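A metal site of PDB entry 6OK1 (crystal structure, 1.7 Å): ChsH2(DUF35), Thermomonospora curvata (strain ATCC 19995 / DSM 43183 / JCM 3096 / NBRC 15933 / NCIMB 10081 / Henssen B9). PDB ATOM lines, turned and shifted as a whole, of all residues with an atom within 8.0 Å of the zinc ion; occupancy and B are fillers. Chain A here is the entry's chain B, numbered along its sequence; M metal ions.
The side-chain hydroxyl of Thr 31 lies close to the side-chain sulfur of Cys 29, at 3.2 Å. N of Ser 45 sits close to SG of Cys 43 (3.6 Å). The side-chain sulfur (SG) of Cys 26 sits close to the backbone NH (N) of Ala 28, 3.4 Å away. The backbone carbonyl oxygen (O) of Thr 31 sits at hydrogen-bond distance from the backbone NH (N) of Cys 26 (3.0 Å). The backbone carbonyl oxygen (O) of Ser 45 lies within hydrogen-bond range of the backbone NH (N) of Cys 40. The backbone NH of His 42 sits close to the side-chain sulfur of Cys 40 (3.4 Å).
The nearest printed residue that does not touch the zinc ion is Ala 28 (4.6 Å).
The zinc ion is bound by the side-chain sulfur of Cys 29 (2.3 Å), the side-chain sulfur of Cys 43 (2.3 Å), the side-chain sulfur of Cys 26 (2.3 Å) and the side-chain sulfur of Cys 40 (2.4 Å). The zinc ion has four donor atoms within binding distance.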
ATOM      1  N   ARG A  25      12.728  21.628  15.538  1.00  0.00           N
ATOM      2  CA  ARG A  25      13.677  21.941  16.590  1.00  0.00           C
ATOM      3  C   ARG A  25      14.749  22.891  16.073  1.00  0.00           C
ATOM      4  O   ARG A  25      15.254  22.719  14.955  1.00  0.00           O
ATOM      5  CB  ARG A  25      14.338  20.678  17.122  1.00  0.00           C
ATOM      6  CG  ARG A  25      15.380  20.937  18.186  1.00  0.00           C
ATOM      7  CD  ARG A  25      15.932  19.625  18.701  1.00  0.00           C
ATOM      8  NE  ARG A  25      16.779  18.980  17.714  1.00  0.00           N
ATOM      9  CZ  ARG A  25      17.493  17.871  17.932  1.00  0.00           C
ATOM     10  NH1 ARG A  25      17.469  17.275  19.116  1.00  0.00           N
ATOM     11  NH2 ARG A  25      18.238  17.358  16.978  1.00  0.00           N
ATOM     12  N   CYS A  26      15.084  23.894  16.888  1.00  0.00           N
ATOM     13  CA  CYS A  26      16.212  24.763  16.582  1.00  0.00           C
ATOM     14  C   CYS A  26      17.508  23.963  16.594  1.00  0.00           C
ATOM     15  O   CYS A  26      17.832  23.292  17.580  1.00  0.00           O
ATOM     16  CB  CYS A  26      16.301  25.900  17.593  1.00  0.00           C
ATOM     17  SG  CYS A  26      17.663  27.029  17.196  1.00  0.00           S
ATOM     18  N   ALA A  27      18.242  24.002  15.495  1.00  0.00           N
ATOM     19  CA  ALA A  27      19.502  23.278  15.438  1.00  0.00           C
ATOM     20  C   ALA A  27      20.567  23.909  16.350  1.00  0.00           C
ATOM     21  O   ALA A  27      21.510  23.228  16.733  1.00  0.00           O
ATOM     22  CB  ALA A  27      20.014  23.210  14.001  1.00  0.00           C
ATOM     23  N   ALA A  28      20.419  25.184  16.701  1.00  0.00           N
ATOM     24  CA  ALA A  28      21.410  25.885  17.524  1.00  0.00           C
ATOM     25  C   ALA A  28      21.183  25.648  19.018  1.00  0.00           C
ATOM     26  O   ALA A  28      22.096  25.212  19.722  1.00  0.00           O
ATOM     27  CB  ALA A  28      21.381  27.385  17.223  1.00  0.00           C
ATOM     28  N   CYS A  29      19.995  25.972  19.518  1.00  0.00           N
ATOM     29  CA  CYS A  29      19.720  25.864  20.937  1.00  0.00           C
ATOM     30  C   CYS A  29      18.873  24.653  21.298  1.00  0.00           C
ATOM     31  O   CYS A  29      18.633  24.436  22.485  1.00  0.00           O
ATOM     32  CB  CYS A  29      19.049  27.150  21.472  1.00  0.00           C
ATOM     33  SG  CYS A  29      17.303  27.337  20.995  1.00  0.00           S
ATOM     34  N   LYS A  30      18.424  23.867  20.305  1.00  0.00           N
ATOM     35  CA  LYS A  30      17.688  22.618  20.483  1.00  0.00           C
ATOM     36  C   LYS A  30      16.309  22.797  21.089  1.00  0.00           C
ATOM     37  O   LYS A  30      15.703  21.813  21.542  1.00  0.00           O
ATOM     38  CB  LYS A  30      18.489  21.617  21.334  1.00  0.00           C
ATOM     39  CG  LYS A  30      19.882  21.400  20.837  1.00  0.00           C
ATOM     40  CD  LYS A  30      19.914  20.798  19.446  1.00  0.00           C
ATOM     41  CE  LYS A  30      21.326  20.307  19.079  1.00  0.00           C
ATOM     42  NZ  LYS A  30      22.302  21.430  18.995  1.00  0.00           N
ATOM     43  N   THR A  31      15.783  24.015  21.107  1.00  0.00           N
ATOM     44  CA  THR A  31      14.422  24.215  21.605  1.00  0.00           C
ATOM     45  C   THR A  31      13.396  23.776  20.550  1.00  0.00           C
ATOM     46  O   THR A  31      13.495  24.142  19.381  1.00  0.00           O
ATOM     47  CB  THR A  31      14.191  25.683  21.981  1.00  0.00           C
ATOM     48  OG1 THR A  31      15.128  26.066  22.999  1.00  0.00           O
ATOM     49  CG2 THR A  31      12.780  25.860  22.514  1.00  0.00           C
ATOM     50  N   LEU A  32      12.414  22.988  20.988  1.00  0.00           N
ATOM     51  CA  LEU A  32      11.332  22.543  20.090  1.00  0.00           C
ATOM     52  C   LEU A  32      10.370  23.673  19.816  1.00  0.00           C
ATOM     53  O   LEU A  32      10.176  24.565  20.646  1.00  0.00           O
ATOM     54  CB  LEU A  32      10.555  21.380  20.707  1.00  0.00           C
ATOM     55  CG  LEU A  32      11.352  20.106  21.049  1.00  0.00           C
ATOM     56  CD1 LEU A  32      10.487  19.012  21.648  1.00  0.00           C
ATOM     57  CD2 LEU A  32      12.063  19.605  19.823  1.00  0.00           C
ATOM     58  N   ARG A  33       9.700  23.599  18.676  1.00  0.00           N
ATOM     59  CA  ARG A  33       8.640  24.556  18.390  1.00  0.00           C
ATOM     60  C   ARG A  33       7.569  23.922  17.530  1.00  0.00           C
ATOM     61  O   ARG A  33       7.867  23.184  16.590  1.00  0.00           O
ATOM     62  CB  ARG A  33       9.184  25.809  17.710  1.00  0.00           C
ATOM     63  CG  ARG A  33       9.968  25.597  16.434  1.00  0.00           C
ATOM     64  CD  ARG A  33      10.434  26.975  15.951  1.00  0.00           C
ATOM     65  NE  ARG A  33      11.093  26.974  14.662  1.00  0.00           N
ATOM     66  CZ  ARG A  33      12.406  27.026  14.461  1.00  0.00           C
ATOM     67  NH1 ARG A  33      13.268  27.034  15.492  1.00  0.00           N
ATOM     68  NH2 ARG A  33      12.862  27.084  13.225  1.00  0.00           N
ATOM     69  N   CYS A  39      12.155  30.359  11.966  1.00  0.00           N
ATOM     70  CA  CYS A  39      13.076  31.011  12.886  1.00  0.00           C
ATOM     71  C   CYS A  39      12.889  30.473  14.301  1.00  0.00           C
ATOM     72  O   CYS A  39      11.815  29.977  14.654  1.00  0.00           O
ATOM     73  CB  CYS A  39      12.832  32.525  12.824  1.00  0.00           C
ATOM     74  SG  CYS A  39      13.952  33.548  13.756  1.00  0.00           S
ATOM     75  N   CYS A  40      13.943  30.543  15.114  1.00  0.00           N
ATOM     76  CA  CYS A  40      13.836  30.207  16.516  1.00  0.00           C
ATOM     77  C   CYS A  40      13.544  31.467  17.336  1.00  0.00           C
ATOM     78  O   CYS A  40      14.355  32.414  17.300  1.00  0.00           O
ATOM     79  CB  CYS A  40      15.122  29.584  17.011  1.00  0.00           C
ATOM     80  SG  CYS A  40      15.043  29.201  18.779  1.00  0.00           S
ATOM     81  N   PRO A  41      12.449  31.512  18.086  1.00  0.00           N
ATOM     82  CA  PRO A  41      12.160  32.723  18.870  1.00  0.00           C
ATOM     83  C   PRO A  41      13.038  32.852  20.105  1.00  0.00           C
ATOM     84  O   PRO A  41      13.034  33.919  20.730  1.00  0.00           O
ATOM     85  CB  PRO A  41      10.694  32.556  19.259  1.00  0.00           C
ATOM     86  CG  PRO A  41      10.510  31.061  19.334  1.00  0.00           C
ATOM     87  CD  PRO A  41      11.339  30.532  18.178  1.00  0.00           C
ATOM     88  N   HIS A  42      13.791  31.818  20.462  1.00  0.00           N
ATOM     89  CA  HIS A  42      14.629  31.874  21.653  1.00  0.00           C
ATOM     90  C   HIS A  42      16.019  32.423  21.363  1.00  0.00           C
ATOM     91  O   HIS A  42      16.532  33.244  22.135  1.00  0.00           O
ATOM     92  CB  HIS A  42      14.674  30.482  22.272  1.00  0.00           C
ATOM     93  CG  HIS A  42      13.303  29.925  22.489  1.00  0.00           C
ATOM     94  ND1 HIS A  42      12.519  30.283  23.567  1.00  0.00           N
ATOM     95  CD2 HIS A  42      12.530  29.129  21.714  1.00  0.00           C
ATOM     96  CE1 HIS A  42      11.350  29.671  23.476  1.00  0.00           C
ATOM     97  NE2 HIS A  42      11.329  28.969  22.364  1.00  0.00           N
ATOM     98  N   CYS A  43      16.615  32.062  20.223  1.00  0.00           N
ATOM     99  CA  CYS A  43      17.990  32.462  19.923  1.00  0.00           C
ATOM    100  C   CYS A  43      18.138  33.131  18.563  1.00  0.00           C
ATOM    101  O   CYS A  43      19.221  33.654  18.275  1.00  0.00           O
ATOM    102  CB  CYS A  43      18.931  31.245  19.993  1.00  0.00           C
ATOM    103  SG  CYS A  43      18.913  30.125  18.584  1.00  0.00           S
ATOM    104  N   GLY A  44      17.094  33.131  17.722  1.00  0.00           N
ATOM    105  CA  GLY A  44      17.119  33.816  16.449  1.00  0.00           C
ATOM    106  C   GLY A  44      17.700  33.026  15.295  1.00  0.00           C
ATOM    107  O   GLY A  44      17.747  33.551  14.178  1.00  0.00           O
ATOM    108  N   SER A  45      18.110  31.785  15.524  1.00  0.00           N
ATOM    109  CA  SER A  45      18.704  30.973  14.462  1.00  0.00           C
ATOM    110  C   SER A  45      17.656  30.611  13.427  1.00  0.00           C
ATOM    111  O   SER A  45      16.514  30.346  13.777  1.00  0.00           O
ATOM    112  CB  SER A  45      19.307  29.704  15.033  1.00  0.00           C
ATOM    113  OG  SER A  45      19.831  28.892  14.000  1.00  0.00           O
ATOM    114  N   PHE A  46      18.066  30.580  12.152  1.00  0.00           N
ATOM    115  CA  PHE A  46      17.237  30.049  11.076  1.00  0.00           C
ATOM    116  C   PHE A  46      17.605  28.621  10.720  1.00  0.00           C
ATOM    117  O   PHE A  46      17.090  28.076   9.738  1.00  0.00           O
ATOM    118  CB  PHE A  46      17.323  30.962   9.836  1.00  0.00           C
ATOM    119  CG  PHE A  46      16.588  32.274  10.002  1.00  0.00           C
ATOM    120  CD1 PHE A  46      17.167  33.324  10.701  1.00  0.00           C
ATOM    121  CD2 PHE A  46      15.316  32.439   9.488  1.00  0.00           C
ATOM    122  CE1 PHE A  46      16.497  34.511  10.861  1.00  0.00           C
ATOM    123  CE2 PHE A  46      14.634  33.640   9.661  1.00  0.00           C
ATOM    124  CZ  PHE A  46      15.220  34.670  10.366  1.00  0.00           C
ATOM    125  N   ASP A  47      18.506  28.003  11.480  1.00  0.00           N
ATOM    126  CA  ASP A  47      18.883  26.622  11.260  1.00  0.00           C
ATOM    127  C   ASP A  47      18.005  25.724  12.135  1.00  0.00           C
ATOM    128  O   ASP A  47      17.880  25.946  13.339  1.00  0.00           O
ATOM    129  CB  ASP A  47      20.363  26.416  11.590  1.00  0.00           C
ATOM    130  CG  ASP A  47      21.285  27.269  10.720  1.00  0.00           C
ATOM    131  OD1 ASP A  47      20.962  27.499   9.537  1.00  0.00           O
ATOM    132  OD2 ASP A  47      22.333  27.713  11.235  1.00  0.00           O
HETATM  133 ZN    ZN M   1      17.295  28.478  19.006  1.00  0.00          ZN
